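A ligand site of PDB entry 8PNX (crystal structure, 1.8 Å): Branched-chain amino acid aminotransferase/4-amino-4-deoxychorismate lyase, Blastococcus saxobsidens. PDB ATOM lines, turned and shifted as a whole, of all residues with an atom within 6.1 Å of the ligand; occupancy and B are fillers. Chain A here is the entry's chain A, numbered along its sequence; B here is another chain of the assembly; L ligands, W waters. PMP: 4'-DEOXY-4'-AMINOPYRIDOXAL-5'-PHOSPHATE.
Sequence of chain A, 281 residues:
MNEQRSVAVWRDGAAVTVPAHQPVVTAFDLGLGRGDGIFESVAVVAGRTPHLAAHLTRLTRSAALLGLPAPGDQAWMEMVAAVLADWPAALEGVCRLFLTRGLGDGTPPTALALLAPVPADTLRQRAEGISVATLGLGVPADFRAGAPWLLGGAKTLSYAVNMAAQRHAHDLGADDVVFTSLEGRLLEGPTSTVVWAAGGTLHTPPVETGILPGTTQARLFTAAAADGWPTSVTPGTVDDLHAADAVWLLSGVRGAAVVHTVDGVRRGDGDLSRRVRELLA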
ATOM      1  N   PHE A  39     -12.059 -24.801  -5.817  1.00  0.00           N
ATOM      2  CA  PHE A  39     -10.748 -25.455  -5.874  1.00  0.00           C
ATOM      3  C   PHE A  39     -10.692 -26.662  -4.950  1.00  0.00           C
ATOM      4  O   PHE A  39     -11.618 -26.965  -4.181  1.00  0.00           O
ATOM      5  CB  PHE A  39      -9.638 -24.480  -5.545  1.00  0.00           C
ATOM      6  CG  PHE A  39      -9.448 -24.240  -4.089  1.00  0.00           C
ATOM      7  CD1 PHE A  39     -10.327 -23.427  -3.392  1.00  0.00           C
ATOM      8  CD2 PHE A  39      -8.388 -24.816  -3.415  1.00  0.00           C
ATOM      9  CE1 PHE A  39     -10.134 -23.150  -2.062  1.00  0.00           C
ATOM     10  CE2 PHE A  39      -8.193 -24.530  -2.071  1.00  0.00           C
ATOM     11  CZ  PHE A  39      -9.060 -23.706  -1.403  1.00  0.00           C
ATOM     12  N   GLU A  40      -9.611 -27.399  -5.163  1.00  0.00           N
ATOM     13  CA  GLU A  40      -9.184 -28.535  -4.317  1.00  0.00           C
ATOM     14  C   GLU A  40      -7.685 -28.428  -4.117  1.00  0.00           C
ATOM     15  O   GLU A  40      -6.967 -27.902  -4.989  1.00  0.00           O
ATOM     16  CB  GLU A  40      -9.527 -29.892  -4.916  1.00  0.00           C
ATOM     17  CG  GLU A  40     -10.994 -30.240  -4.771  1.00  0.00           C
ATOM     18  CD  GLU A  40     -11.370 -30.551  -3.333  1.00  0.00           C
ATOM     19  OE1 GLU A  40     -10.470 -30.918  -2.540  1.00  0.00           O
ATOM     20  OE2 GLU A  40     -12.527 -30.349  -3.004  1.00  0.00           O
ATOM     21  N   SER A  41      -7.221 -28.843  -2.946  1.00  0.00           N
ATOM     22  CA  SER A  41      -5.783 -28.873  -2.593  1.00  0.00           C
ATOM     23  C   SER A  41      -5.381 -30.332  -2.391  1.00  0.00           C
ATOM     24  O   SER A  41      -5.984 -30.991  -1.545  1.00  0.00           O
ATOM     25  CB  SER A  41      -5.456 -28.032  -1.383  1.00  0.00           C
ATOM     26  OG  SER A  41      -5.746 -26.647  -1.586  1.00  0.00           O
ATOM     27  N   HIS A  55     -10.538 -36.007  -3.590  1.00  0.00           N
ATOM     28  CA  HIS A  55     -10.543 -34.562  -3.957  1.00  0.00           C
ATOM     29  C   HIS A  55     -11.343 -34.361  -5.232  1.00  0.00           C
ATOM     30  O   HIS A  55     -12.114 -33.359  -5.287  1.00  0.00           O
ATOM     31  CB  HIS A  55      -9.117 -34.024  -4.066  1.00  0.00           C
ATOM     32  CG  HIS A  55      -8.461 -33.974  -2.735  1.00  0.00           C
ATOM     33  ND1 HIS A  55      -8.711 -32.995  -1.821  1.00  0.00           N
ATOM     34  CD2 HIS A  55      -7.506 -34.769  -2.207  1.00  0.00           C
ATOM     35  CE1 HIS A  55      -7.980 -33.203  -0.747  1.00  0.00           C
ATOM     36  NE2 HIS A  55      -7.237 -34.309  -0.966  1.00  0.00           N
ATOM     37  N   ARG A  58     -15.073 -34.464  -4.506  1.00  0.00           N
ATOM     38  CA  ARG A  58     -15.553 -33.211  -3.868  1.00  0.00           C
ATOM     39  C   ARG A  58     -15.543 -32.023  -4.842  1.00  0.00           C
ATOM     40  O   ARG A  58     -16.458 -31.156  -4.722  1.00  0.00           O
ATOM     41  CB  ARG A  58     -14.741 -32.860  -2.632  1.00  0.00           C
ATOM     42  CG  ARG A  58     -15.362 -31.689  -1.879  1.00  0.00           C
ATOM     43  CD  ARG A  58     -14.690 -31.420  -0.515  1.00  0.00           C
ATOM     44  NE  ARG A  58     -13.267 -31.130  -0.660  1.00  0.00           N
ATOM     45  CZ  ARG A  58     -12.402 -31.219   0.360  1.00  0.00           C
ATOM     46  NH1 ARG A  58     -12.827 -31.545   1.573  1.00  0.00           N
ATOM     47  NH2 ARG A  58     -11.108 -31.042   0.155  1.00  0.00           N
ATOM     48  N   LYS A 155     -16.262 -25.505  -1.672  1.00  0.00           N
ATOM     49  CA  LYS A 155     -14.875 -25.064  -1.477  1.00  0.00           C
ATOM     50  C   LYS A 155     -14.544 -24.088  -2.607  1.00  0.00           C
ATOM     51  O   LYS A 155     -14.252 -24.567  -3.693  1.00  0.00           O
ATOM     52  CB  LYS A 155     -13.966 -26.288  -1.484  1.00  0.00           C
ATOM     53  CG  LYS A 155     -12.565 -26.034  -0.996  1.00  0.00           C
ATOM     54  CD  LYS A 155     -11.739 -27.316  -0.799  1.00  0.00           C
ATOM     55  CE  LYS A 155     -10.278 -26.984  -0.846  1.00  0.00           C
ATOM     56  NZ  LYS A 155      -9.997 -25.960   0.187  1.00  0.00           N
ATOM     57  N   TYR A 159     -11.994 -16.931  -0.323  1.00  0.00           N
ATOM     58  CA  TYR A 159     -11.500 -17.239   1.058  1.00  0.00           C
ATOM     59  C   TYR A 159     -10.962 -15.973   1.726  1.00  0.00           C
ATOM     60  O   TYR A 159     -10.110 -16.114   2.616  1.00  0.00           O
ATOM     61  CB  TYR A 159     -10.396 -18.299   1.051  1.00  0.00           C
ATOM     62  CG  TYR A 159     -10.834 -19.721   1.295  1.00  0.00           C
ATOM     63  CD1 TYR A 159     -11.811 -20.304   0.515  1.00  0.00           C
ATOM     64  CD2 TYR A 159     -10.205 -20.538   2.228  1.00  0.00           C
ATOM     65  CE1 TYR A 159     -12.171 -21.642   0.658  1.00  0.00           C
ATOM     66  CE2 TYR A 159     -10.569 -21.879   2.406  1.00  0.00           C
ATOM     67  CZ  TYR A 159     -11.535 -22.450   1.583  1.00  0.00           C
ATOM     68  OH  TYR A 159     -12.001 -23.734   1.718  1.00  0.00           O
ATOM     69  N   ASN A 162     -11.650 -16.225   5.471  1.00  0.00           N
ATOM     70  CA  ASN A 162     -10.826 -17.393   5.931  1.00  0.00           C
ATOM     71  C   ASN A 162      -9.416 -16.896   6.198  1.00  0.00           C
ATOM     72  O   ASN A 162      -8.918 -17.127   7.298  1.00  0.00           O
ATOM     73  CB  ASN A 162     -10.790 -18.517   4.899  1.00  0.00           C
ATOM     74  CG  ASN A 162     -12.173 -18.989   4.525  1.00  0.00           C
ATOM     75  OD1 ASN A 162     -12.979 -18.199   4.005  1.00  0.00           O
ATOM     76  ND2 ASN A 162     -12.449 -20.258   4.793  1.00  0.00           N
ATOM     77  N   GLU A 188     -15.761 -25.224  11.750  1.00  0.00           N
ATOM     78  CA  GLU A 188     -14.529 -25.807  11.199  1.00  0.00           C
ATOM     79  C   GLU A 188     -13.455 -24.735  11.253  1.00  0.00           C
ATOM     80  O   GLU A 188     -13.764 -23.572  11.615  1.00  0.00           O
ATOM     81  CB  GLU A 188     -14.780 -26.266   9.764  1.00  0.00           C
ATOM     82  CG  GLU A 188     -15.071 -25.100   8.837  1.00  0.00           C
ATOM     83  CD  GLU A 188     -15.523 -25.536   7.456  1.00  0.00           C
ATOM     84  OE1 GLU A 188     -14.992 -26.570   6.984  1.00  0.00           O
ATOM     85  OE2 GLU A 188     -16.422 -24.840   6.868  1.00  0.00           O
ATOM     86  N   GLY A 189     -12.250 -25.116  10.881  1.00  0.00           N
ATOM     87  CA  GLY A 189     -11.146 -24.160  10.683  1.00  0.00           C
ATOM     88  C   GLY A 189     -11.316 -23.427   9.363  1.00  0.00           C
ATOM     89  O   GLY A 189     -12.043 -23.891   8.469  1.00  0.00           O
ATOM     90  N   PRO A 190     -10.589 -22.309   9.181  1.00  0.00           N
ATOM     91  CA  PRO A 190     -10.585 -21.584   7.902  1.00  0.00           C
ATOM     92  C   PRO A 190     -10.150 -22.474   6.728  1.00  0.00           C
ATOM     93  O   PRO A 190     -10.553 -22.156   5.631  1.00  0.00           O
ATOM     94  CB  PRO A 190      -9.571 -20.440   8.130  1.00  0.00           C
ATOM     95  CG  PRO A 190      -9.504 -20.286   9.598  1.00  0.00           C
ATOM     96  CD  PRO A 190      -9.712 -21.666  10.180  1.00  0.00           C
ATOM     97  N   THR A 191      -9.333 -23.498   6.977  1.00  0.00           N
ATOM     98  CA  THR A 191      -8.735 -24.403   5.965  1.00  0.00           C
ATOM     99  C   THR A 191      -8.654 -25.821   6.526  1.00  0.00           C
ATOM    100  O   THR A 191      -7.840 -26.599   5.972  1.00  0.00           O
ATOM    101  CB  THR A 191      -7.349 -23.924   5.508  1.00  0.00           C
ATOM    102  OG1 THR A 191      -6.404 -24.068   6.567  1.00  0.00           O
ATOM    103  CG2 THR A 191      -7.325 -22.492   4.995  1.00  0.00           C
ATOM    104  N   SER A 192      -9.479 -26.199   7.494  1.00  0.00           N
ATOM    105  CA  SER A 192      -9.327 -27.497   8.184  1.00  0.00           C
ATOM    106  C   SER A 192     -10.584 -27.898   8.934  1.00  0.00           C
ATOM    107  O   SER A 192     -11.513 -27.056   9.146  1.00  0.00           O
ATOM    108  CB  SER A 192      -8.126 -27.503   9.122  1.00  0.00           C
ATOM    109  OG  SER A 192      -8.327 -26.576  10.206  1.00  0.00           O
ATOM    110  N   THR A 193     -10.594 -29.172   9.320  1.00  0.00           N
ATOM    111  CA  THR A 193     -11.715 -29.825  10.006  1.00  0.00           C
ATOM    112  C   THR A 193     -11.326 -30.022  11.460  1.00  0.00           C
ATOM    113  O   THR A 193     -10.223 -30.516  11.715  1.00  0.00           O
ATOM    114  CB  THR A 193     -12.076 -31.168   9.366  1.00  0.00           C
ATOM    115  OG1 THR A 193     -12.441 -30.917   8.013  1.00  0.00           O
ATOM    116  CG2 THR A 193     -13.223 -31.842  10.097  1.00  0.00           C
ATOM    117  N   LEU A 212     -17.467 -27.485   5.229  1.00  0.00           N
ATOM    118  CA  LEU A 212     -16.912 -28.408   4.206  1.00  0.00           C
ATOM    119  C   LEU A 212     -16.795 -29.818   4.785  1.00  0.00           C
ATOM    120  O   LEU A 212     -16.211 -29.991   5.868  1.00  0.00           O
ATOM    121  CB  LEU A 212     -15.552 -27.878   3.768  1.00  0.00           C
ATOM    122  CG  LEU A 212     -14.998 -28.454   2.467  1.00  0.00           C
ATOM    123  CD1 LEU A 212     -15.883 -28.024   1.271  1.00  0.00           C
ATOM    124  CD2 LEU A 212     -13.548 -28.032   2.270  1.00  0.00           C
ATOM    125  N   PRO A 213     -17.248 -30.852   4.038  1.00  0.00           N
ATOM    126  CA  PRO A 213     -17.020 -32.255   4.423  1.00  0.00           C
ATOM    127  C   PRO A 213     -15.549 -32.601   4.156  1.00  0.00           C
ATOM    128  O   PRO A 213     -15.135 -32.661   3.027  1.00  0.00           O
ATOM    129  CB  PRO A 213     -17.972 -33.082   3.526  1.00  0.00           C
ATOM    130  CG  PRO A 213     -18.664 -32.084   2.624  1.00  0.00           C
ATOM    131  CD  PRO A 213     -17.945 -30.764   2.754  1.00  0.00           C
ATOM    132  N   GLY A 214     -14.774 -32.720   5.218  1.00  0.00           N
ATOM    133  CA  GLY A 214     -13.317 -32.864   5.114  1.00  0.00           C
ATOM    134  C   GLY A 214     -12.961 -34.287   4.718  1.00  0.00           C
ATOM    135  O   GLY A 214     -13.396 -35.254   5.410  1.00  0.00           O
ATOM    136  N   THR A 215     -12.073 -34.403   3.750  1.00  0.00           N
ATOM    137  CA  THR A 215     -11.632 -35.732   3.246  1.00  0.00           C
ATOM    138  C   THR A 215     -10.656 -36.356   4.266  1.00  0.00           C
ATOM    139  O   THR A 215     -10.676 -37.577   4.435  1.00  0.00           O
ATOM    140  CB  THR A 215     -11.056 -35.640   1.827  1.00  0.00           C
ATOM    141  OG1 THR A 215      -9.833 -34.906   1.919  1.00  0.00           O
ATOM    142  CG2 THR A 215     -12.020 -34.989   0.858  1.00  0.00           C
ATOM    143  N   THR A 216      -9.799 -35.571   4.912  1.00  0.00           N
ATOM    144  CA  THR A 216      -8.863 -36.113   5.927  1.00  0.00           C
ATOM    145  C   THR A 216      -9.664 -36.646   7.132  1.00  0.00           C
ATOM    146  O   THR A 216      -9.305 -37.712   7.675  1.00  0.00           O
ATOM    147  CB  THR A 216      -7.813 -35.071   6.351  1.00  0.00           C
ATOM    148  OG1 THR A 216      -7.278 -34.404   5.227  1.00  0.00           O
ATOM    149  CG2 THR A 216      -6.682 -35.706   7.122  1.00  0.00           C
ATOM    150  N   GLN A 217     -10.611 -35.880   7.640  1.00  0.00           N
ATOM    151  CA  GLN A 217     -11.489 -36.345   8.757  1.00  0.00           C
ATOM    152  C   GLN A 217     -12.282 -37.596   8.333  1.00  0.00           C
ATOM    153  O   GLN A 217     -12.337 -38.542   9.120  1.00  0.00           O
ATOM    154  CB  GLN A 217     -12.400 -35.218   9.228  1.00  0.00           C
ATOM    155  CG  GLN A 217     -13.474 -35.658  10.207  1.00  0.00           C
ATOM    156  CD  GLN A 217     -14.728 -36.189   9.562  1.00  0.00           C
ATOM    157  OE1 GLN A 217     -15.313 -35.538   8.701  1.00  0.00           O
ATOM    158  NE2 GLN A 217     -15.129 -37.372   9.988  1.00  0.00           N
ATOM    159  N   LEU A 250      -7.540 -31.116  11.112  1.00  0.00           N
ATOM    160  CA  LEU A 250      -7.163 -32.037  10.005  1.00  0.00           C
ATOM    161  C   LEU A 250      -7.417 -31.379   8.652  1.00  0.00           C
ATOM    162  O   LEU A 250      -8.518 -30.799   8.466  1.00  0.00           O
ATOM    163  CB  LEU A 250      -8.046 -33.294  10.079  1.00  0.00           C
ATOM    164  CG  LEU A 250      -8.134 -33.970  11.432  1.00  0.00           C
ATOM    165  CD1 LEU A 250      -8.854 -35.259  11.276  1.00  0.00           C
ATOM    166  CD2 LEU A 250      -6.783 -34.194  12.073  1.00  0.00           C
ATOM    167  N   SER A 251      -6.468 -31.529   7.733  1.00  0.00           N
ATOM    168  CA  SER A 251      -6.523 -31.037   6.346  1.00  0.00           C
ATOM    169  C   SER A 251      -5.591 -31.850   5.459  1.00  0.00           C
ATOM    170  O   SER A 251      -4.655 -32.502   5.962  1.00  0.00           O
ATOM    171  CB  SER A 251      -6.224 -29.579   6.272  1.00  0.00           C
ATOM    172  OG  SER A 251      -4.939 -29.334   6.805  1.00  0.00           O
ATOM    173  N   GLY A 252      -5.873 -31.814   4.142  1.00  0.00           N
ATOM    174  CA  GLY A 252      -5.169 -32.665   3.181  1.00  0.00           C
ATOM    175  C   GLY A 252      -3.734 -32.256   3.049  1.00  0.00           C
ATOM    176  O   GLY A 252      -2.932 -33.131   2.782  1.00  0.00           O
ATOM    177  N   VAL A 253      -3.398 -30.999   3.288  1.00  0.00           N
ATOM    178  CA  VAL A 253      -2.010 -30.484   3.081  1.00  0.00           C
ATOM    179  C   VAL A 253      -1.278 -30.526   4.421  1.00  0.00           C
ATOM    180  O   VAL A 253      -0.268 -31.268   4.513  1.00  0.00           O
ATOM    181  CB  VAL A 253      -1.960 -29.077   2.472  1.00  0.00           C
ATOM    182  CG1 VAL A 253      -0.540 -28.559   2.370  1.00  0.00           C
ATOM    183  CG2 VAL A 253      -2.635 -28.996   1.115  1.00  0.00           C
ATOM    184  N   ARG B  34      -7.277 -17.319  -3.393  1.00  0.00           N
ATOM    185  CA  ARG B  34      -7.947 -17.050  -2.094  1.00  0.00           C
ATOM    186  C   ARG B  34      -8.979 -15.907  -2.181  1.00  0.00           C
ATOM    187  O   ARG B  34      -9.579 -15.595  -1.148  1.00  0.00           O
ATOM    188  CB  ARG B  34      -6.876 -16.737  -1.047  1.00  0.00           C
ATOM    189  CG  ARG B  34      -6.013 -17.939  -0.699  1.00  0.00           C
ATOM    190  CD  ARG B  34      -6.781 -19.037   0.035  1.00  0.00           C
ATOM    191  NE  ARG B  34      -5.889 -20.170   0.370  1.00  0.00           N
ATOM    192  CZ  ARG B  34      -6.263 -21.358   0.858  1.00  0.00           C
ATOM    193  NH1 ARG B  34      -7.525 -21.657   1.059  1.00  0.00           N
ATOM    194  NH2 ARG B  34      -5.341 -22.258   1.133  1.00  0.00           N
HETATM  195  N1  PMP L   1     -12.587 -26.794   5.780  1.00  0.00           N
HETATM  196  C2  PMP L   1     -12.164 -25.887   4.909  1.00  0.00           C
HETATM  197  C2A PMP L   1     -12.873 -24.568   4.889  1.00  0.00           C
HETATM  198  C3  PMP L   1     -11.062 -26.178   4.074  1.00  0.00           C
HETATM  199  O3  PMP L   1     -10.602 -25.222   3.209  1.00  0.00           O
HETATM  200  C4  PMP L   1     -10.453 -27.436   4.156  1.00  0.00           C
HETATM  201  C4A PMP L   1      -9.257 -27.778   3.282  1.00  0.00           C
HETATM  202  N4A PMP L   1      -9.757 -28.197   1.978  1.00  0.00           N
HETATM  203  C5  PMP L   1     -10.934 -28.366   5.096  1.00  0.00           C
HETATM  204  C6  PMP L   1     -12.011 -27.992   5.862  1.00  0.00           C
HETATM  205  C5A PMP L   1     -10.325 -29.720   5.279  1.00  0.00           C
HETATM  206  O4P PMP L   1     -10.549 -30.578   4.116  1.00  0.00           O
HETATM  207  P   PMP L   1      -9.437 -31.657   3.567  1.00  0.00           P
HETATM  208  O1P PMP L   1      -8.159 -30.994   3.116  1.00  0.00           O
HETATM  209  O2P PMP L   1      -9.301 -32.576   4.815  1.00  0.00           O
HETATM  210  O3P PMP L   1     -10.178 -32.339   2.447  1.00  0.00           O
HETATM  211  O   HOH W   1     -10.656 -33.001   6.916  1.00  0.00           O
HETATM  212  O   HOH W   2      -7.832 -30.229   0.609  1.00  0.00           O
HETATM  213  O   HOH W   3      -5.541 -28.909   2.404  1.00  0.00           O
HETATM  214  O   HOH W   4     -14.875 -23.841   2.167  1.00  0.00           O
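OH of Tyr 159 lies within hydrogen-bond range of O3 of the ligand (2.5 Å). The backbone NH (N) of Gly 252 is in hydrogen-bond range of an oxygen (O1P) of the ligand (2.6 Å). O3P of the ligand sits at hydrogen-bond distance from N of Thr 215 (3.1 Å). An oxygen (O3P) of the ligand is in hydrogen-bond range of the side-chain hydroxyl (OG1) of Thr 215, 2.6 Å away. The side-chain carboxylate (OE1) of Glu 188 sits at hydrogen-bond distance from a nitrogen (N1) of the ligand (2.7 Å). O2P of the ligand sits at hydrogen-bond distance from N of Thr 216, at 3.0 Å. The side-chain hydroxyl (OG1) of Thr 216 lies within hydrogen-bond range of an oxygen (O2P) of the ligand (2.8 Å). NH2 of Arg 58 lies within salt-bridge range of O3P of the ligand (2.8 Å). O3 of the ligand lies within hydrogen-bond range of NZ of Lys 155 (3.2 Å).
The backbone NH (N) of Tyr 159 is in hydrogen-bond range of the backbone carbonyl oxygen (O) of Arg 34 of chain B (2.9 Å). OG1 of Thr 216 sits at hydrogen-bond distance from N of Gly 252, 3.1 Å away. The guanidinium group (NH1) of Arg 58 is in hydrogen-bond range of the backbone carbonyl oxygen (O) of Pro 213 (2.9 Å). NE of Arg 58 is in salt-bridge range of OE2 of Glu 40, 2.6 Å away. The backbone NH (N) of Phe 39 lies within hydrogen-bond range of the backbone carbonyl oxygen (O) of Lys 155 (3.1 Å). ND2 of Asn 162 sits at hydrogen-bond distance from O of Pro 190 (2.8 Å). The backbone NH of Thr 193 is in hydrogen-bond range of the backbone carbonyl oxygen of Leu 250, at 2.8 Å. The side-chain carboxylate of Glu 40 is in hydrogen-bond range of a ring nitrogen (ND1) of His 55 (2.8 Å).
His 55 touches the ligand (CE1 to O3P, 3.97 Å). Gly 189 touches the ligand (O to C2A, 3.7 Å). Pro 190 touches the ligand (O to C2A, 3.4 Å). Thr 191 touches the ligand. Ser 192 touches the ligand. Thr 193 touches the ligand (OG1 to C6, 3.7 Å). Leu 212 touches the ligand. Gly 214 touches the ligand. O of Leu 250 touches C5A of the ligand, at 3.8 Å. Ser 251 touches the ligand. Hydrophobic or aromatic side chains within 4 Å of the ligand: His 55, Tyr 159 and Leu 212. Within 4 Å of the ligand: His 55, Arg 58, Lys 155, Tyr 159, Glu 188, Gly 189, Pro 190, Thr 191, Ser 192, Thr 193, Leu 212, Gly 214, Thr 215, Thr 216, Leu 250, Ser 251 and Gly 252. The nearest printed residue that does not touch the ligand is Asn 162 (4.3 Å).
Water W1 lies within hydrogen-bond range of an oxygen (O2P) of the ligand (2.5 Å), the side-chain hydroxyl of Thr 193 (3.0 Å), the backbone NH of Gln 217 (3.0 Å), the backbone NH of Thr 216 (3.4 Å) and the backbone carbonyl oxygen of Leu 250 (3.4 Å). Water W2 lies within hydrogen-bond range of an oxygen (O1P) of the ligand (2.6 Å), the backbone carbonyl oxygen (O) of Ser 41 (2.9 Å) and the guanidinium group (NH2) of Arg 58 (3.4 Å). Water W3 lies within hydrogen-bond range of N of Val 253, N of Gly 252 and O1P of the ligand.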
